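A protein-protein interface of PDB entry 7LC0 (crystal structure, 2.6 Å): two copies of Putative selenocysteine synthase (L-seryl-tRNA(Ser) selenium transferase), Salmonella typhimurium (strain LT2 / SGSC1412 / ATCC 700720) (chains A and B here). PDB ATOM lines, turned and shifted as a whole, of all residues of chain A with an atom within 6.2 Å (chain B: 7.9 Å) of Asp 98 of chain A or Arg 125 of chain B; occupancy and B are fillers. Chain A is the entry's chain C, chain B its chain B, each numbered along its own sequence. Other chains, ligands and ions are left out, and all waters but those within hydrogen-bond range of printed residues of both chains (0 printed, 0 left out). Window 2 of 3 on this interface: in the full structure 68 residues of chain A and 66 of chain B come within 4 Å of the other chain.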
ATOM      1  N   ARG A  92      29.061 -34.250   1.867  1.00  0.00           N
ATOM      2  CA  ARG A  92      29.300 -34.364   3.300  1.00  0.00           C
ATOM      3  C   ARG A  92      29.618 -33.010   3.923  1.00  0.00           C
ATOM      4  O   ARG A  92      29.312 -32.784   5.099  1.00  0.00           O
ATOM      5  CB  ARG A  92      30.428 -35.361   3.561  1.00  0.00           C
ATOM      6  CG  ARG A  92      30.105 -36.777   3.106  1.00  0.00           C
ATOM      7  CD  ARG A  92      31.212 -37.742   3.480  1.00  0.00           C
ATOM      8  NE  ARG A  92      30.707 -39.095   3.691  1.00  0.00           N
ATOM      9  CZ  ARG A  92      31.296 -39.996   4.470  1.00  0.00           C
ATOM     10  NH1 ARG A  92      32.409 -39.687   5.120  1.00  0.00           N
ATOM     11  NH2 ARG A  92      30.769 -41.206   4.605  1.00  0.00           N
ATOM     12  N   VAL A  93      30.229 -32.102   3.158  1.00  0.00           N
ATOM     13  CA  VAL A  93      30.466 -30.753   3.661  1.00  0.00           C
ATOM     14  C   VAL A  93      29.143 -30.029   3.884  1.00  0.00           C
ATOM     15  O   VAL A  93      28.982 -29.281   4.856  1.00  0.00           O
ATOM     16  CB  VAL A  93      31.388 -29.979   2.699  1.00  0.00           C
ATOM     17  CG1 VAL A  93      31.398 -28.495   3.035  1.00  0.00           C
ATOM     18  CG2 VAL A  93      32.804 -30.538   2.754  1.00  0.00           C
ATOM     19  N   ALA A  94      28.167 -30.258   3.002  1.00  0.00           N
ATOM     20  CA  ALA A  94      26.873 -29.600   3.145  1.00  0.00           C
ATOM     21  C   ALA A  94      26.114 -30.098   4.369  1.00  0.00           C
ATOM     22  O   ALA A  94      25.339 -29.341   4.965  1.00  0.00           O
ATOM     23  CB  ALA A  94      26.039 -29.806   1.881  1.00  0.00           C
ATOM     24  N   LEU A  95      26.321 -31.357   4.763  1.00  0.00           N
ATOM     25  CA  LEU A  95      25.603 -31.910   5.905  1.00  0.00           C
ATOM     26  C   LEU A  95      26.186 -31.478   7.242  1.00  0.00           C
ATOM     27  O   LEU A  95      25.499 -31.589   8.263  1.00  0.00           O
ATOM     28  CB  LEU A  95      25.582 -33.437   5.831  1.00  0.00           C
ATOM     29  CG  LEU A  95      24.466 -34.064   4.997  1.00  0.00           C
ATOM     30  CD1 LEU A  95      24.505 -35.577   5.126  1.00  0.00           C
ATOM     31  CD2 LEU A  95      23.112 -33.519   5.427  1.00  0.00           C
ATOM     32  N   MET A  96      27.424 -30.997   7.262  1.00  0.00           N
ATOM     33  CA  MET A  96      28.066 -30.587   8.508  1.00  0.00           C
ATOM     34  C   MET A  96      27.282 -29.475   9.191  1.00  0.00           C
ATOM     35  O   MET A  96      26.740 -28.597   8.521  1.00  0.00           O
ATOM     36  CB  MET A  96      29.501 -30.133   8.243  1.00  0.00           C
ATOM     37  CG  MET A  96      30.430 -31.237   7.761  1.00  0.00           C
ATOM     38  SD  MET A  96      30.718 -32.670   9.063  1.00  0.00           S
ATOM     39  CE  MET A  96      29.321 -33.911   8.498  1.00  0.00           C
ATOM     40  N   PRO A  97      27.232 -29.501  10.533  1.00  0.00           N
ATOM     41  CA  PRO A  97      27.919 -30.468  11.396  1.00  0.00           C
ATOM     42  C   PRO A  97      27.112 -31.719  11.750  1.00  0.00           C
ATOM     43  O   PRO A  97      27.358 -32.300  12.807  1.00  0.00           O
ATOM     44  CB  PRO A  97      28.190 -29.652  12.658  1.00  0.00           C
ATOM     45  CG  PRO A  97      27.012 -28.741  12.742  1.00  0.00           C
ATOM     46  CD  PRO A  97      26.625 -28.409  11.317  1.00  0.00           C
ATOM     47  N   ASP A  98      26.181 -32.136  10.894  1.00  0.00           N
ATOM     48  CA  ASP A  98      25.384 -33.336  11.156  1.00  0.00           C
ATOM     49  C   ASP A  98      26.068 -34.530  10.501  1.00  0.00           C
ATOM     50  O   ASP A  98      25.925 -34.763   9.299  1.00  0.00           O
ATOM     51  CB  ASP A  98      23.956 -33.167  10.652  1.00  0.00           C
ATOM     52  CG  ASP A  98      23.103 -34.394  10.914  1.00  0.00           C
ATOM     53  OD1 ASP A  98      23.227 -34.981  12.009  1.00  0.00           O
ATOM     54  OD2 ASP A  98      22.304 -34.767  10.029  1.00  0.00           O
ATOM     55  N   SER A  99      26.806 -35.296  11.303  1.00  0.00           N
ATOM     56  CA  SER A  99      27.503 -36.482  10.823  1.00  0.00           C
ATOM     57  C   SER A  99      26.859 -37.740  11.391  1.00  0.00           C
ATOM     58  O   SER A  99      27.539 -38.573  11.998  1.00  0.00           O
ATOM     59  CB  SER A  99      28.979 -36.420  11.211  1.00  0.00           C
ATOM     60  OG  SER A  99      29.114 -36.246  12.610  1.00  0.00           O
ATOM     61  N   SER A 100      25.547 -37.888  11.183  1.00  0.00           N
ATOM     62  CA  SER A 100      24.803 -38.947  11.860  1.00  0.00           C
ATOM     63  C   SER A 100      25.234 -40.333  11.391  1.00  0.00           C
ATOM     64  O   SER A 100      25.350 -41.258  12.204  1.00  0.00           O
ATOM     65  CB  SER A 100      23.300 -38.752  11.644  1.00  0.00           C
ATOM     66  OG  SER A 100      22.860 -37.517  12.189  1.00  0.00           O
ATOM     67  N   GLY A 101      25.475 -40.502  10.093  1.00  0.00           N
ATOM     68  CA  GLY A 101      25.794 -41.805   9.548  1.00  0.00           C
ATOM     69  C   GLY A 101      27.238 -42.011   9.160  1.00  0.00           C
ATOM     70  O   GLY A 101      27.548 -43.010   8.494  1.00  0.00           O
ATOM     71  N   MET A 102      28.136 -41.116   9.551  1.00  0.00           N
ATOM     72  CA  MET A 102      29.529 -41.195   9.138  1.00  0.00           C
ATOM     73  C   MET A 102      30.460 -41.512  10.304  1.00  0.00           C
ATOM     74  O   MET A 102      30.051 -41.492  11.465  1.00  0.00           O
ATOM     75  CB  MET A 102      29.955 -39.881   8.486  1.00  0.00           C
ATOM     76  CG  MET A 102      29.035 -39.421   7.375  1.00  0.00           C
ATOM     77  SD  MET A 102      28.908 -37.480   7.296  1.00  0.00           S
ATOM     78  CE  MET A 102      30.747 -37.066   6.843  1.00  0.00           C
ATOM     79  N   GLY A 128      31.424 -31.425  13.452  1.00  0.00           N
ATOM     80  CA  GLY A 128      30.728 -32.694  13.377  1.00  0.00           C
ATOM     81  C   GLY A 128      31.401 -33.836  14.101  1.00  0.00           C
ATOM     82  O   GLY A 128      31.078 -34.996  13.841  1.00  0.00           O
ATOM     83  N   ILE B  77      23.699 -15.608  11.773  1.00  0.00           N
ATOM     84  CA  ILE B  77      22.585 -16.546  11.683  1.00  0.00           C
ATOM     85  C   ILE B  77      22.767 -17.682  12.681  1.00  0.00           C
ATOM     86  O   ILE B  77      21.828 -18.063  13.391  1.00  0.00           O
ATOM     87  CB  ILE B  77      22.443 -17.070  10.243  1.00  0.00           C
ATOM     88  CG1 ILE B  77      22.163 -15.910   9.284  1.00  0.00           C
ATOM     89  CG2 ILE B  77      21.336 -18.109  10.159  1.00  0.00           C
ATOM     90  CD1 ILE B  77      22.083 -16.324   7.828  1.00  0.00           C
ATOM     91  N   ALA B  78      23.982 -18.230  12.762  1.00  0.00           N
ATOM     92  CA  ALA B  78      24.240 -19.324  13.695  1.00  0.00           C
ATOM     93  C   ALA B  78      24.112 -18.862  15.141  1.00  0.00           C
ATOM     94  O   ALA B  78      23.563 -19.584  15.982  1.00  0.00           O
ATOM     95  CB  ALA B  78      25.627 -19.912  13.439  1.00  0.00           C
ATOM     96  N   VAL B  81      20.379 -18.229  15.962  1.00  0.00           N
ATOM     97  CA  VAL B  81      19.668 -19.492  16.134  1.00  0.00           C
ATOM     98  C   VAL B  81      20.064 -20.148  17.450  1.00  0.00           C
ATOM     99  O   VAL B  81      19.210 -20.652  18.191  1.00  0.00           O
ATOM    100  CB  VAL B  81      19.922 -20.415  14.929  1.00  0.00           C
ATOM    101  CG1 VAL B  81      19.460 -21.828  15.235  1.00  0.00           C
ATOM    102  CG2 VAL B  81      19.205 -19.880  13.700  1.00  0.00           C
ATOM    103  N   ILE B  85      17.654 -21.143  20.785  1.00  0.00           N
ATOM    104  CA  ILE B  85      17.566 -22.495  21.328  1.00  0.00           C
ATOM    105  C   ILE B  85      18.053 -22.545  22.769  1.00  0.00           C
ATOM    106  O   ILE B  85      17.413 -23.161  23.625  1.00  0.00           O
ATOM    107  CB  ILE B  85      18.363 -23.462  20.431  1.00  0.00           C
ATOM    108  CG1 ILE B  85      17.794 -23.461  19.009  1.00  0.00           C
ATOM    109  CG2 ILE B  85      18.358 -24.869  21.015  1.00  0.00           C
ATOM    110  CD1 ILE B  85      18.558 -24.354  18.052  1.00  0.00           C
ATOM    111  N   MET B  96      25.908 -26.773  22.189  1.00  0.00           N
ATOM    112  CA  MET B  96      25.730 -26.472  20.770  1.00  0.00           C
ATOM    113  C   MET B  96      26.903 -26.988  19.941  1.00  0.00           C
ATOM    114  O   MET B  96      28.038 -27.004  20.415  1.00  0.00           O
ATOM    115  CB  MET B  96      25.560 -24.966  20.565  1.00  0.00           C
ATOM    116  CG  MET B  96      24.331 -24.372  21.236  1.00  0.00           C
ATOM    117  SD  MET B  96      22.642 -25.126  20.602  1.00  0.00           S
ATOM    118  CE  MET B  96      22.357 -26.472  21.986  1.00  0.00           C
ATOM    119  N   PRO B  97      26.635 -27.412  18.694  1.00  0.00           N
ATOM    120  CA  PRO B  97      25.321 -27.409  18.040  1.00  0.00           C
ATOM    121  C   PRO B  97      24.472 -28.653  18.303  1.00  0.00           C
ATOM    122  O   PRO B  97      23.509 -28.884  17.572  1.00  0.00           O
ATOM    123  CB  PRO B  97      25.685 -27.322  16.560  1.00  0.00           C
ATOM    124  CG  PRO B  97      26.969 -28.068  16.470  1.00  0.00           C
ATOM    125  CD  PRO B  97      27.708 -27.783  17.755  1.00  0.00           C
ATOM    126  N   ASP B  98      24.816 -29.442  19.319  1.00  0.00           N
ATOM    127  CA  ASP B  98      24.032 -30.628  19.660  1.00  0.00           C
ATOM    128  C   ASP B  98      22.825 -30.181  20.474  1.00  0.00           C
ATOM    129  O   ASP B  98      22.869 -30.092  21.701  1.00  0.00           O
ATOM    130  CB  ASP B  98      24.876 -31.644  20.422  1.00  0.00           C
ATOM    131  CG  ASP B  98      24.135 -32.947  20.676  1.00  0.00           C
ATOM    132  OD1 ASP B  98      23.006 -33.109  20.166  1.00  0.00           O
ATOM    133  OD2 ASP B  98      24.682 -33.814  21.389  1.00  0.00           O
ATOM    134  N   SER B  99      21.727 -29.896  19.773  1.00  0.00           N
ATOM    135  CA  SER B  99      20.484 -29.456  20.391  1.00  0.00           C
ATOM    136  C   SER B  99      19.483 -30.594  20.551  1.00  0.00           C
ATOM    137  O   SER B  99      18.270 -30.358  20.559  1.00  0.00           O
ATOM    138  CB  SER B  99      19.866 -28.320  19.579  1.00  0.00           C
ATOM    139  OG  SER B  99      19.611 -28.737  18.249  1.00  0.00           O
ATOM    140  N   VAL B 106      13.711 -24.450  13.380  1.00  0.00           N
ATOM    141  CA  VAL B 106      13.719 -23.102  12.823  1.00  0.00           C
ATOM    142  C   VAL B 106      12.743 -23.087  11.656  1.00  0.00           C
ATOM    143  O   VAL B 106      13.008 -23.670  10.599  1.00  0.00           O
ATOM    144  CB  VAL B 106      15.123 -22.679  12.379  1.00  0.00           C
ATOM    145  CG1 VAL B 106      15.093 -21.268  11.807  1.00  0.00           C
ATOM    146  CG2 VAL B 106      16.096 -22.771  13.544  1.00  0.00           C
ATOM    147  N   PRO B 119      24.900 -22.835   1.626  1.00  0.00           N
ATOM    148  CA  PRO B 119      23.469 -22.907   1.944  1.00  0.00           C
ATOM    149  C   PRO B 119      23.180 -22.318   3.317  1.00  0.00           C
ATOM    150  O   PRO B 119      23.932 -22.522   4.273  1.00  0.00           O
ATOM    151  CB  PRO B 119      23.168 -24.408   1.895  1.00  0.00           C
ATOM    152  CG  PRO B 119      24.484 -25.066   2.142  1.00  0.00           C
ATOM    153  CD  PRO B 119      25.510 -24.170   1.511  1.00  0.00           C
ATOM    154  N   VAL B 120      22.076 -21.570   3.402  1.00  0.00           N
ATOM    155  CA  VAL B 120      21.696 -20.929   4.656  1.00  0.00           C
ATOM    156  C   VAL B 120      21.394 -21.957   5.737  1.00  0.00           C
ATOM    157  O   VAL B 120      21.475 -21.644   6.929  1.00  0.00           O
ATOM    158  CB  VAL B 120      20.495 -19.984   4.429  1.00  0.00           C
ATOM    159  CG1 VAL B 120      19.221 -20.780   4.187  1.00  0.00           C
ATOM    160  CG2 VAL B 120      20.328 -19.028   5.602  1.00  0.00           C
ATOM    161  N   THR B 121      21.061 -23.191   5.349  1.00  0.00           N
ATOM    162  CA  THR B 121      20.815 -24.233   6.339  1.00  0.00           C
ATOM    163  C   THR B 121      22.089 -24.621   7.077  1.00  0.00           C
ATOM    164  O   THR B 121      22.022 -25.070   8.227  1.00  0.00           O
ATOM    165  CB  THR B 121      20.199 -25.463   5.672  1.00  0.00           C
ATOM    166  OG1 THR B 121      21.085 -25.950   4.656  1.00  0.00           O
ATOM    167  CG2 THR B 121      18.861 -25.112   5.046  1.00  0.00           C
ATOM    168  N   SER B 122      23.250 -24.463   6.439  1.00  0.00           N
ATOM    169  CA  SER B 122      24.509 -24.789   7.103  1.00  0.00           C
ATOM    170  C   SER B 122      24.750 -23.869   8.293  1.00  0.00           C
ATOM    171  O   SER B 122      25.127 -24.323   9.379  1.00  0.00           O
ATOM    172  CB  SER B 122      25.667 -24.706   6.108  1.00  0.00           C
ATOM    173  OG  SER B 122      25.589 -25.744   5.146  1.00  0.00           O
ATOM    174  N   ALA B 123      24.533 -22.564   8.106  1.00  0.00           N
ATOM    175  CA  ALA B 123      24.665 -21.631   9.219  1.00  0.00           C
ATOM    176  C   ALA B 123      23.623 -21.911  10.295  1.00  0.00           C
ATOM    177  O   ALA B 123      23.917 -21.828  11.493  1.00  0.00           O
ATOM    178  CB  ALA B 123      24.548 -20.192   8.715  1.00  0.00           C
ATOM    179  N   ILE B 124      22.398 -22.247   9.885  1.00  0.00           N
ATOM    180  CA  ILE B 124      21.361 -22.593  10.853  1.00  0.00           C
ATOM    181  C   ILE B 124      21.730 -23.872  11.592  1.00  0.00           C
ATOM    182  O   ILE B 124      21.547 -23.977  12.811  1.00  0.00           O
ATOM    183  CB  ILE B 124      19.998 -22.720  10.149  1.00  0.00           C
ATOM    184  CG1 ILE B 124      19.623 -21.400   9.477  1.00  0.00           C
ATOM    185  CG2 ILE B 124      18.924 -23.139  11.139  1.00  0.00           C
ATOM    186  CD1 ILE B 124      18.459 -21.520   8.523  1.00  0.00           C
ATOM    187  N   ARG B 125      22.261 -24.861  10.869  1.00  0.00           N
ATOM    188  CA  ARG B 125      22.649 -26.113  11.506  1.00  0.00           C
ATOM    189  C   ARG B 125      23.809 -25.915  12.474  1.00  0.00           C
ATOM    190  O   ARG B 125      23.918 -26.645  13.464  1.00  0.00           O
ATOM    191  CB  ARG B 125      23.013 -27.152  10.445  1.00  0.00           C
ATOM    192  CG  ARG B 125      23.022 -28.581  10.956  1.00  0.00           C
ATOM    193  CD  ARG B 125      23.391 -29.573   9.861  1.00  0.00           C
ATOM    194  NE  ARG B 125      22.483 -29.508   8.718  1.00  0.00           N
ATOM    195  CZ  ARG B 125      22.791 -28.956   7.549  1.00  0.00           C
ATOM    196  NH1 ARG B 125      23.990 -28.422   7.360  1.00  0.00           N
ATOM    197  NH2 ARG B 125      21.900 -28.941   6.566  1.00  0.00           N
ATOM    198  N   LEU B 126      24.676 -24.933  12.209  1.00  0.00           N
ATOM    199  CA  LEU B 126      25.772 -24.648  13.129  1.00  0.00           C
ATOM    200  C   LEU B 126      25.264 -24.106  14.458  1.00  0.00           C
ATOM    201  O   LEU B 126      25.933 -24.266  15.485  1.00  0.00           O
ATOM    202  CB  LEU B 126      26.752 -23.661  12.495  1.00  0.00           C
ATOM    203  CG  LEU B 126      27.766 -24.264  11.522  1.00  0.00           C
ATOM    204  CD1 LEU B 126      28.648 -23.179  10.930  1.00  0.00           C
ATOM    205  CD2 LEU B 126      28.605 -25.315  12.230  1.00  0.00           C
ATOM    206  N   GLY B 127      24.100 -23.462  14.458  1.00  0.00           N
ATOM    207  CA  GLY B 127      23.472 -23.001  15.675  1.00  0.00           C
ATOM    208  C   GLY B 127      22.641 -24.039  16.389  1.00  0.00           C
ATOM    209  O   GLY B 127      21.999 -23.724  17.393  1.00  0.00           O
ATOM    210  N   GLY B 128      22.636 -25.276  15.900  1.00  0.00           N
ATOM    211  CA  GLY B 128      21.841 -26.332  16.488  1.00  0.00           C
ATOM    212  C   GLY B 128      20.413 -26.412  16.000  1.00  0.00           C
ATOM    213  O   GLY B 128      19.610 -27.134  16.602  1.00  0.00           O
ATOM    214  N   GLY B 129      20.071 -25.701  14.930  1.00  0.00           N
ATOM    215  CA  GLY B 129      18.704 -25.664  14.455  1.00  0.00           C
ATOM    216  C   GLY B 129      18.400 -26.744  13.431  1.00  0.00           C
ATOM    217  O   GLY B 129      19.281 -27.224  12.723  1.00  0.00           O
ATOM    218  N   ARG B 130      17.125 -27.122  13.368  1.00  0.00           N
ATOM    219  CA  ARG B 130      16.621 -28.066  12.380  1.00  0.00           C
ATOM    220  C   ARG B 130      15.598 -27.357  11.505  1.00  0.00           C
ATOM    221  O   ARG B 130      14.702 -26.678  12.017  1.00  0.00           O
ATOM    222  CB  ARG B 130      15.998 -29.295  13.048  1.00  0.00           C
ATOM    223  CG  ARG B 130      16.987 -30.130  13.845  1.00  0.00           C
ATOM    224  CD  ARG B 130      16.328 -31.373  14.416  1.00  0.00           C
ATOM    225  NE  ARG B 130      15.761 -32.217  13.369  1.00  0.00           N
ATOM    226  CZ  ARG B 130      15.151 -33.377  13.593  1.00  0.00           C
ATOM    227  NH1 ARG B 130      15.031 -33.836  14.831  1.00  0.00           N
ATOM    228  NH2 ARG B 130      14.666 -34.079  12.578  1.00  0.00           N
ATOM    229  N   ILE B 131      15.731 -27.521  10.194  1.00  0.00           N
ATOM    230  CA  ILE B 131      14.924 -26.771   9.238  1.00  0.00           C
ATOM    231  C   ILE B 131      13.518 -27.347   9.182  1.00  0.00           C
ATOM    232  O   ILE B 131      13.325 -28.568   9.136  1.00  0.00           O
ATOM    233  CB  ILE B 131      15.586 -26.787   7.848  1.00  0.00           C
ATOM    234  CG1 ILE B 131      17.025 -26.288   7.946  1.00  0.00           C
ATOM    235  CG2 ILE B 131      14.800 -25.929   6.869  1.00  0.00           C
ATOM    236  CD1 ILE B 131      17.130 -24.879   8.458  1.00  0.00           C
ATOM    237  N   ILE B 240      29.789 -21.613  20.599  1.00  0.00           N
ATOM    238  CA  ILE B 240      30.107 -21.705  19.178  1.00  0.00           C
ATOM    239  C   ILE B 240      30.659 -20.403  18.612  1.00  0.00           C
ATOM    240  O   ILE B 240      31.349 -20.430  17.585  1.00  0.00           O
ATOM    241  CB  ILE B 240      28.874 -22.134  18.367  1.00  0.00           C
ATOM    242  CG1 ILE B 240      27.785 -21.063  18.439  1.00  0.00           C
ATOM    243  CG2 ILE B 240      28.345 -23.461  18.878  1.00  0.00           C
ATOM    244  CD1 ILE B 240      26.597 -21.343  17.546  1.00  0.00           C
ATOM    245  N   MET B 244      33.836 -18.384  15.609  1.00  0.00           N
ATOM    246  CA  MET B 244      33.456 -17.361  14.645  1.00  0.00           C
ATOM    247  C   MET B 244      33.942 -16.007  15.138  1.00  0.00           C
ATOM    248  O   MET B 244      33.189 -15.034  15.172  1.00  0.00           O
ATOM    249  CB  MET B 244      31.942 -17.351  14.447  1.00  0.00           C
ATOM    250  CG  MET B 244      31.352 -18.732  14.233  1.00  0.00           C
ATOM    251  SD  MET B 244      29.436 -18.801  14.568  1.00  0.00           S
ATOM    252  CE  MET B 244      29.165 -20.722  14.359  1.00  0.00           C
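NH1 of Arg 125 of chain B is in hydrogen-bond range of O of Ala 94 of chain A (2.9 Å). The guanidinium group of Arg 125 of chain B is in hydrogen-bond range of the backbone carbonyl oxygen of Met 96 of chain A (3.0 Å).
The side-chain hydroxyl (OG) of Ser 100 of chain A lies within hydrogen-bond range of the side-chain carboxylate (OD1) of Asp 98 of chain A, 2.6 Å away.
Asp 98 of chain A touches just one residue of chain B: Arg 125 (3.7 Å). Arg 125 of chain B touches five residues of chain A. Of the printed residues of chain B, Pro 97 of chain A touches Pro 97, Arg 125 and Leu 126. Printed residues of chain A within 4 Å of Pro 97 of chain B: Pro 97 (3.8 Å). Of the printed residues of chain A, Leu 126 of chain B touches Pro 97 (3.8 Å). Of the printed residues of chain A, Ser 122 of chain B touches Ala 94. Of the printed residues of chain B, Ala 94 of chain A touches Ser 122 (3.6 Å) and Arg 125 (2.9 Å). Ser 99 of chain B touches none of the printed residues of chain A. Val 106 of chain B touches none of the printed residues of chain A. The nearest residue of chain A that does not touch Arg 125 of chain B is Val 93 of chain A (5.7 Å). The nearest printed residue of chain B that does not touch Leu 95 of chain A is Ser 122 of chain B (5.7 Å).
Pro 97 of chain B touches its own counterpart, Pro 97 of chain A. Positions printed for both chains: 96, 97, 98, 99 and 128. Of the 8 pairs that touch across the chains among the printed residues, 1 has its exchanged pair printed and touching as well.
Hydrophobic or aromatic side chains of chain A that line the printed part of chain B: Pro 97.
Among the printed residues, pairs that only touch across the chains: Leu 95 of chain A with Arg 125 of chain B (3.3 Å), Ala 94 of chain A with Ser 122 of chain B (3.6 Å), Pro 97 of chain A with Arg 125 of chain B (3.6 Å), Asp 98 of chain A with Arg 125 of chain B (3.7 Å), Pro 97 of chain A with Leu 126 of chain B (3.8 Å) and Pro 97 of chain A with Pro 97 of chain B (3.8 Å).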
